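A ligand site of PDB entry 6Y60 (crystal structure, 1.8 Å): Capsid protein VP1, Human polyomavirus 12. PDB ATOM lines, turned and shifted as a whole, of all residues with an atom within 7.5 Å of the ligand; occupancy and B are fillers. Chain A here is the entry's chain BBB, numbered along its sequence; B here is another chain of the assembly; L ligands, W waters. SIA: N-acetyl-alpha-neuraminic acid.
The backbone carbonyl oxygen (O) of Thr 54 sits close to an oxygen (O10) of the ligand (3.3 Å).
Ala 49 touches the ligand.
Thr 50 touches the ligand.
CA of Asp 55 touches O10 of the ligand (3.7 Å).
Pro 57 touches the ligand (N to C11, 3.9 Å).
His 106 of chain B touches the ligand (O to C11, 3.7 Å).
Of the 24 residues printed, 10 come within 4 Å of the ligand.
The side-chain carboxylate of Asp 55 is in hydrogen-bond range of a ring nitrogen (ND1) of His 106 of chain B (2.7 Å).
The backbone carbonyl oxygen of Gly 115 of chain B sits at hydrogen-bond distance from the guanidinium group of Arg 111 of chain B (3.0 Å).
OG1 of Thr 47 sits at hydrogen-bond distance from OE1 of Gln 61 (3.0 Å).
O of Asn 114 of chain B sits at hydrogen-bond distance from NH2 of Arg 111 of chain B (3.0 Å).
OD2 of Asp 55 lies close to OD1 of Asp 107 of chain B.
The backbone carbonyl oxygen (O) of Asp 55 sits at hydrogen-bond distance from the backbone NH (N) of Gln 147.
The backbone carbonyl oxygen (O) of His 106 of chain B is in hydrogen-bond range of the backbone NH (N) of Ala 49, 2.8 Å away.
N of Arg 56 lies within hydrogen-bond range of O10 of the ligand (2.9 Å).
The backbone carbonyl oxygen (O) of Val 48 sits at hydrogen-bond distance from an oxygen (O7) of the ligand (2.7 Å).
N of Val 48 is in hydrogen-bond range of O9 of the ligand (3.0 Å).
The guanidinium group (NH1) of Arg 111 of chain B lies within hydrogen-bond range of an oxygen (O9) of the ligand (2.8 Å).
A nitrogen (N5) of the ligand is in hydrogen-bond range of the side-chain hydroxyl of Thr 47, at 2.9 Å.
The backbone carbonyl oxygen (O) of Arg 56 sits at hydrogen-bond distance from an oxygen (O4) of the ligand.
Water W3 lies within hydrogen-bond range of O4 of the ligand and O of Thr 54.
Water W1 lies within hydrogen-bond range of an oxygen (O4) of the ligand and the backbone carbonyl oxygen of Arg 56.
Water W2 lies within hydrogen-bond range of O9 of the ligand (2.8 Å) and NH2 of Arg 111 of chain B (3.1 Å).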
ATOM      1  N   GLN A  45      13.233  -9.820  -6.428  1.00  0.00           N
ATOM      2  CA  GLN A  45      12.696 -10.169  -5.092  1.00  0.00           C
ATOM      3  C   GLN A  45      12.408 -11.661  -5.039  1.00  0.00           C
ATOM      4  O   GLN A  45      11.684 -12.183  -5.887  1.00  0.00           O
ATOM      5  CB  GLN A  45      11.490  -9.278  -4.793  1.00  0.00           C
ATOM      6  CG  GLN A  45      11.912  -7.824  -4.621  1.00  0.00           C
ATOM      7  CD  GLN A  45      10.785  -6.970  -4.095  1.00  0.00           C
ATOM      8  OE1 GLN A  45       9.623  -7.361  -4.136  1.00  0.00           O
ATOM      9  NE2 GLN A  45      11.129  -5.820  -3.537  1.00  0.00           N
ATOM     10  N   VAL A  46      12.978 -12.364  -4.044  1.00  0.00           N
ATOM     11  CA  VAL A  46      12.803 -13.837  -3.938  1.00  0.00           C
ATOM     12  C   VAL A  46      11.402 -14.183  -3.410  1.00  0.00           C
ATOM     13  O   VAL A  46      11.045 -13.729  -2.306  1.00  0.00           O
ATOM     14  CB  VAL A  46      13.898 -14.478  -3.064  1.00  0.00           C
ATOM     15  CG1 VAL A  46      13.559 -15.922  -2.725  1.00  0.00           C
ATOM     16  CG2 VAL A  46      15.245 -14.384  -3.755  1.00  0.00           C
ATOM     17  N   THR A  47      10.698 -15.066  -4.108  1.00  0.00           N
ATOM     18  CA  THR A  47       9.394 -15.588  -3.671  1.00  0.00           C
ATOM     19  C   THR A  47       9.647 -17.004  -3.167  1.00  0.00           C
ATOM     20  O   THR A  47      10.598 -17.673  -3.646  1.00  0.00           O
ATOM     21  CB  THR A  47       8.334 -15.504  -4.794  1.00  0.00           C
ATOM     22  OG1 THR A  47       8.578 -16.497  -5.792  1.00  0.00           O
ATOM     23  CG2 THR A  47       8.286 -14.141  -5.451  1.00  0.00           C
ATOM     24  N   VAL A  48       8.756 -17.447  -2.301  1.00  0.00           N
ATOM     25  CA  VAL A  48       8.873 -18.749  -1.599  1.00  0.00           C
ATOM     26  C   VAL A  48       7.620 -19.546  -1.886  1.00  0.00           C
ATOM     27  O   VAL A  48       6.531 -18.962  -1.777  1.00  0.00           O
ATOM     28  CB  VAL A  48       9.039 -18.488  -0.092  1.00  0.00           C
ATOM     29  CG1 VAL A  48       9.034 -19.774   0.720  1.00  0.00           C
ATOM     30  CG2 VAL A  48      10.284 -17.660   0.174  1.00  0.00           C
ATOM     31  N   ALA A  49       7.768 -20.854  -2.098  1.00  0.00           N
ATOM     32  CA  ALA A  49       6.664 -21.788  -2.400  1.00  0.00           C
ATOM     33  C   ALA A  49       5.696 -21.869  -1.217  1.00  0.00           C
ATOM     34  O   ALA A  49       6.172 -21.858  -0.071  1.00  0.00           O
ATOM     35  CB  ALA A  49       7.230 -23.157  -2.725  1.00  0.00           C
ATOM     36  N   THR A  50       4.407 -22.051  -1.474  1.00  0.00           N
ATOM     37  CA  THR A  50       3.361 -22.299  -0.443  1.00  0.00           C
ATOM     38  C   THR A  50       3.121 -23.799  -0.340  1.00  0.00           C
ATOM     39  O   THR A  50       2.351 -24.263   0.544  1.00  0.00           O
ATOM     40  CB  THR A  50       2.095 -21.507  -0.753  1.00  0.00           C
ATOM     41  OG1 THR A  50       1.607 -21.998  -2.005  1.00  0.00           O
ATOM     42  CG2 THR A  50       2.340 -20.013  -0.837  1.00  0.00           C
ATOM     43  N   ALA A  51       3.743 -24.568  -1.210  1.00  0.00           N
ATOM     44  CA  ALA A  51       3.709 -26.042  -1.117  1.00  0.00           C
ATOM     45  C   ALA A  51       4.886 -26.620  -1.892  1.00  0.00           C
ATOM     46  O   ALA A  51       5.379 -25.988  -2.870  1.00  0.00           O
ATOM     47  CB  ALA A  51       2.388 -26.576  -1.628  1.00  0.00           C
ATOM     48  N   THR A  54       4.052 -27.108  -5.697  1.00  0.00           N
ATOM     49  CA  THR A  54       3.735 -25.881  -6.481  1.00  0.00           C
ATOM     50  C   THR A  54       4.966 -24.973  -6.520  1.00  0.00           C
ATOM     51  O   THR A  54       4.838 -23.763  -6.818  1.00  0.00           O
ATOM     52  CB  THR A  54       2.511 -25.178  -5.893  1.00  0.00           C
ATOM     53  OG1 THR A  54       2.938 -24.285  -4.854  1.00  0.00           O
ATOM     54  CG2 THR A  54       1.466 -26.127  -5.352  1.00  0.00           C
ATOM     55  N   ASP A  55       6.144 -25.538  -6.268  1.00  0.00           N
ATOM     56  CA  ASP A  55       7.383 -24.775  -6.052  1.00  0.00           C
ATOM     57  C   ASP A  55       7.973 -24.445  -7.408  1.00  0.00           C
ATOM     58  O   ASP A  55       8.667 -25.319  -7.974  1.00  0.00           O
ATOM     59  CB  ASP A  55       8.311 -25.612  -5.177  1.00  0.00           C
ATOM     60  CG  ASP A  55       9.638 -24.992  -4.825  1.00  0.00           C
ATOM     61  OD1 ASP A  55       9.930 -23.832  -5.242  1.00  0.00           O
ATOM     62  OD2 ASP A  55      10.383 -25.688  -4.097  1.00  0.00           O
ATOM     63  N   ARG A  56       7.805 -23.197  -7.856  1.00  0.00           N
ATOM     64  CA  ARG A  56       8.150 -22.771  -9.240  1.00  0.00           C
ATOM     65  C   ARG A  56       8.922 -21.462  -9.168  1.00  0.00           C
ATOM     66  O   ARG A  56       8.338 -20.392  -9.268  1.00  0.00           O
ATOM     67  CB  ARG A  56       6.910 -22.672 -10.131  1.00  0.00           C
ATOM     68  CG  ARG A  56       6.100 -23.959 -10.175  1.00  0.00           C
ATOM     69  N   PRO A  57      10.262 -21.504  -8.995  1.00  0.00           N
ATOM     70  CA  PRO A  57      11.055 -20.284  -8.967  1.00  0.00           C
ATOM     71  C   PRO A  57      11.088 -19.661 -10.352  1.00  0.00           C
ATOM     72  O   PRO A  57      11.513 -20.309 -11.297  1.00  0.00           O
ATOM     73  CB  PRO A  57      12.473 -20.734  -8.587  1.00  0.00           C
ATOM     74  CG  PRO A  57      12.510 -22.235  -8.865  1.00  0.00           C
ATOM     75  CD  PRO A  57      11.068 -22.725  -8.879  1.00  0.00           C
ATOM     76  N   PRO A  58      10.640 -18.392 -10.509  1.00  0.00           N
ATOM     77  CA  PRO A  58      10.948 -17.614 -11.707  1.00  0.00           C
ATOM     78  C   PRO A  58      12.463 -17.539 -11.907  1.00  0.00           C
ATOM     79  O   PRO A  58      13.172 -17.525 -10.925  1.00  0.00           O
ATOM     80  CB  PRO A  58      10.354 -16.220 -11.390  1.00  0.00           C
ATOM     81  CG  PRO A  58       9.221 -16.548 -10.438  1.00  0.00           C
ATOM     82  CD  PRO A  58       9.750 -17.677  -9.589  1.00  0.00           C
ATOM     83  N   GLN A  61      14.977 -15.044 -10.134  1.00  0.00           N
ATOM     84  CA  GLN A  61      14.993 -15.102  -8.649  1.00  0.00           C
ATOM     85  C   GLN A  61      16.018 -16.117  -8.113  1.00  0.00           C
ATOM     86  O   GLN A  61      16.040 -16.323  -6.879  1.00  0.00           O
ATOM     87  CB  GLN A  61      13.596 -15.412  -8.143  1.00  0.00           C
ATOM     88  CG  GLN A  61      12.652 -14.241  -8.380  1.00  0.00           C
ATOM     89  CD  GLN A  61      11.228 -14.594  -8.033  1.00  0.00           C
ATOM     90  OE1 GLN A  61      10.985 -15.448  -7.176  1.00  0.00           O
ATOM     91  NE2 GLN A  61      10.285 -13.948  -8.706  1.00  0.00           N
ATOM     92  N   VAL A 146      10.751 -29.499  -7.448  1.00  0.00           N
ATOM     93  CA  VAL A 146      10.809 -28.123  -8.009  1.00  0.00           C
ATOM     94  C   VAL A 146      10.465 -28.203  -9.501  1.00  0.00           C
ATOM     95  O   VAL A 146      10.894 -29.169 -10.159  1.00  0.00           O
ATOM     96  CB  VAL A 146      12.167 -27.453  -7.745  1.00  0.00           C
ATOM     97  CG1 VAL A 146      12.284 -26.072  -8.394  1.00  0.00           C
ATOM     98  CG2 VAL A 146      12.418 -27.357  -6.247  1.00  0.00           C
ATOM     99  N   GLN A 147       9.680 -27.236  -9.971  1.00  0.00           N
ATOM    100  CA  GLN A 147       9.340 -27.044 -11.399  1.00  0.00           C
ATOM    101  C   GLN A 147      10.159 -25.856 -11.895  1.00  0.00           C
ATOM    102  O   GLN A 147       9.798 -24.718 -11.554  1.00  0.00           O
ATOM    103  CB  GLN A 147       7.822 -26.854 -11.557  1.00  0.00           C
ATOM    104  CG  GLN A 147       6.989 -28.088 -11.181  1.00  0.00           C
ATOM    105  CD  GLN A 147       5.526 -27.792 -10.909  1.00  0.00           C
ATOM    106  OE1 GLN A 147       5.034 -26.686 -11.096  1.00  0.00           O
ATOM    107  NE2 GLN A 147       4.818 -28.803 -10.429  1.00  0.00           N
ATOM    108  N   HIS A 256      11.091  -7.983   1.359  1.00  0.00           N
ATOM    109  CA  HIS A 256      11.442  -8.812   0.160  1.00  0.00           C
ATOM    110  C   HIS A 256      12.963  -8.806   0.013  1.00  0.00           C
ATOM    111  O   HIS A 256      13.592  -7.747   0.235  1.00  0.00           O
ATOM    112  CB  HIS A 256      10.731  -8.281  -1.102  1.00  0.00           C
ATOM    113  CG  HIS A 256       9.254  -8.442  -1.090  1.00  0.00           C
ATOM    114  ND1 HIS A 256       8.652  -9.632  -1.424  1.00  0.00           N
ATOM    115  CD2 HIS A 256       8.254  -7.599  -0.760  1.00  0.00           C
ATOM    116  CE1 HIS A 256       7.338  -9.509  -1.352  1.00  0.00           C
ATOM    117  NE2 HIS A 256       7.070  -8.272  -0.938  1.00  0.00           N
ATOM    118  N   VAL B 105      16.505 -21.063  -1.391  1.00  0.00           N
ATOM    119  CA  VAL B 105      15.660 -20.463  -0.325  1.00  0.00           C
ATOM    120  C   VAL B 105      14.256 -20.123  -0.841  1.00  0.00           C
ATOM    121  O   VAL B 105      13.574 -19.263  -0.228  1.00  0.00           O
ATOM    122  CB  VAL B 105      16.377 -19.258   0.288  1.00  0.00           C
ATOM    123  CG1 VAL B 105      17.572 -19.737   1.134  1.00  0.00           C
ATOM    124  CG2 VAL B 105      16.818 -18.253  -0.786  1.00  0.00           C
ATOM    125  N   HIS B 106      13.796 -20.841  -1.859  1.00  0.00           N
ATOM    126  CA  HIS B 106      12.460 -20.649  -2.481  1.00  0.00           C
ATOM    127  C   HIS B 106      11.593 -21.888  -2.227  1.00  0.00           C
ATOM    128  O   HIS B 106      10.384 -21.850  -2.531  1.00  0.00           O
ATOM    129  CB  HIS B 106      12.590 -20.320  -3.971  1.00  0.00           C
ATOM    130  CG  HIS B 106      13.071 -21.489  -4.760  1.00  0.00           C
ATOM    131  ND1 HIS B 106      12.305 -22.641  -4.903  1.00  0.00           N
ATOM    132  CD2 HIS B 106      14.244 -21.710  -5.389  1.00  0.00           C
ATOM    133  CE1 HIS B 106      13.017 -23.537  -5.555  1.00  0.00           C
ATOM    134  NE2 HIS B 106      14.196 -22.996  -5.891  1.00  0.00           N
ATOM    135  N   ASP B 107      12.181 -22.936  -1.669  1.00  0.00           N
ATOM    136  CA  ASP B 107      11.408 -24.156  -1.324  1.00  0.00           C
ATOM    137  C   ASP B 107      10.345 -23.780  -0.286  1.00  0.00           C
ATOM    138  O   ASP B 107      10.413 -22.686   0.301  1.00  0.00           O
ATOM    139  CB  ASP B 107      12.323 -25.280  -0.838  1.00  0.00           C
ATOM    140  CG  ASP B 107      13.135 -26.009  -1.904  1.00  0.00           C
ATOM    141  OD1 ASP B 107      12.704 -26.047  -3.114  1.00  0.00           O
ATOM    142  OD2 ASP B 107      14.172 -26.612  -1.511  1.00  0.00           O
ATOM    143  N   TYR B 108       9.427 -24.711  -0.030  1.00  0.00           N
ATOM    144  CA  TYR B 108       8.346 -24.574   0.970  1.00  0.00           C
ATOM    145  C   TYR B 108       9.003 -24.679   2.358  1.00  0.00           C
ATOM    146  O   TYR B 108       9.114 -25.787   2.886  1.00  0.00           O
ATOM    147  CB  TYR B 108       7.255 -25.609   0.708  1.00  0.00           C
ATOM    148  CG  TYR B 108       6.078 -25.530   1.648  1.00  0.00           C
ATOM    149  CD1 TYR B 108       5.566 -24.310   2.052  1.00  0.00           C
ATOM    150  CD2 TYR B 108       5.547 -26.666   2.218  1.00  0.00           C
ATOM    151  CE1 TYR B 108       4.521 -24.234   2.959  1.00  0.00           C
ATOM    152  CE2 TYR B 108       4.479 -26.618   3.089  1.00  0.00           C
ATOM    153  CZ  TYR B 108       3.978 -25.389   3.482  1.00  0.00           C
ATOM    154  OH  TYR B 108       2.928 -25.292   4.354  1.00  0.00           O
ATOM    155  N   ARG B 111       9.622 -18.665   6.754  1.00  0.00           N
ATOM    156  CA  ARG B 111      10.155 -17.352   6.336  1.00  0.00           C
ATOM    157  C   ARG B 111       9.799 -16.283   7.354  1.00  0.00           C
ATOM    158  O   ARG B 111       8.853 -16.468   8.100  1.00  0.00           O
ATOM    159  CB  ARG B 111       9.647 -16.997   4.936  1.00  0.00           C
ATOM    160  CG  ARG B 111       8.159 -16.743   4.834  1.00  0.00           C
ATOM    161  CD  ARG B 111       7.700 -16.810   3.353  1.00  0.00           C
ATOM    162  NE  ARG B 111       8.363 -15.781   2.567  1.00  0.00           N
ATOM    163  CZ  ARG B 111       7.936 -15.282   1.418  1.00  0.00           C
ATOM    164  NH1 ARG B 111       6.808 -15.714   0.882  1.00  0.00           N
ATOM    165  NH2 ARG B 111       8.643 -14.324   0.824  1.00  0.00           N
ATOM    166  N   ASP B 113       8.331 -12.645   7.389  1.00  0.00           N
ATOM    167  CA  ASP B 113       7.628 -11.624   6.560  1.00  0.00           C
ATOM    168  C   ASP B 113       7.752 -12.078   5.082  1.00  0.00           C
ATOM    169  O   ASP B 113       7.393 -13.226   4.797  1.00  0.00           O
ATOM    170  CB  ASP B 113       8.219 -10.235   6.863  1.00  0.00           C
ATOM    171  CG  ASP B 113       8.169  -9.808   8.324  1.00  0.00           C
ATOM    172  OD1 ASP B 113       7.202 -10.192   9.013  1.00  0.00           O
ATOM    173  OD2 ASP B 113       9.100  -9.075   8.768  1.00  0.00           O
ATOM    174  N   ASN B 114       8.295 -11.234   4.202  1.00  0.00           N
ATOM    175  CA  ASN B 114       8.437 -11.522   2.740  1.00  0.00           C
ATOM    176  C   ASN B 114       9.908 -11.873   2.449  1.00  0.00           C
ATOM    177  O   ASN B 114      10.313 -11.852   1.246  1.00  0.00           O
ATOM    178  CB  ASN B 114       7.986 -10.327   1.893  1.00  0.00           C
ATOM    179  CG  ASN B 114       6.480 -10.284   1.782  1.00  0.00           C
ATOM    180  OD1 ASN B 114       5.866 -11.343   1.632  1.00  0.00           O
ATOM    181  ND2 ASN B 114       5.878  -9.112   1.913  1.00  0.00           N
ATOM    182  N   GLY B 115      10.662 -12.190   3.499  1.00  0.00           N
ATOM    183  CA  GLY B 115      12.068 -12.636   3.366  1.00  0.00           C
ATOM    184  C   GLY B 115      12.199 -14.035   2.785  1.00  0.00           C
ATOM    185  O   GLY B 115      11.187 -14.729   2.578  1.00  0.00           O
HETATM  186  C1  SIA L   1       4.454 -15.362  -7.734  1.00  0.00           C
HETATM  187  C2  SIA L   1       3.642 -16.628  -7.459  1.00  0.00           C
HETATM  188  C3  SIA L   1       4.109 -17.803  -8.344  1.00  0.00           C
HETATM  189  C4  SIA L   1       5.479 -18.413  -7.948  1.00  0.00           C
HETATM  190  C5  SIA L   1       5.608 -18.670  -6.424  1.00  0.00           C
HETATM  191  C6  SIA L   1       5.173 -17.388  -5.739  1.00  0.00           C
HETATM  192  C7  SIA L   1       5.257 -17.416  -4.218  1.00  0.00           C
HETATM  193  C8  SIA L   1       4.550 -16.203  -3.606  1.00  0.00           C
HETATM  194  C9  SIA L   1       4.838 -16.135  -2.104  1.00  0.00           C
HETATM  195  C10 SIA L   1       7.447 -20.151  -5.912  1.00  0.00           C
HETATM  196  C11 SIA L   1       8.912 -20.201  -5.535  1.00  0.00           C
HETATM  197  N5  SIA L   1       6.984 -18.934  -6.060  1.00  0.00           N
HETATM  198  O1A SIA L   1       5.097 -15.201  -8.811  1.00  0.00           O
HETATM  199  O1B SIA L   1       4.547 -14.452  -6.899  1.00  0.00           O
HETATM  200  O2  SIA L   1       2.224 -16.393  -7.660  1.00  0.00           O
HETATM  201  O4  SIA L   1       5.651 -19.653  -8.630  1.00  0.00           O
HETATM  202  O6  SIA L   1       3.820 -17.167  -6.154  1.00  0.00           O
HETATM  203  O7  SIA L   1       4.669 -18.632  -3.734  1.00  0.00           O
HETATM  204  O8  SIA L   1       4.962 -14.980  -4.248  1.00  0.00           O
HETATM  205  O9  SIA L   1       6.236 -15.779  -1.896  1.00  0.00           O
HETATM  206  O10 SIA L   1       6.758 -21.143  -6.023  1.00  0.00           O
HETATM  207  O   HOH W   1       5.729 -19.736 -11.347  1.00  0.00           O
HETATM  208  O   HOH W   2       7.208 -13.205  -1.625  1.00  0.00           O
HETATM  209  O   HOH W   3       4.149 -21.420  -7.869  1.00  0.00           O
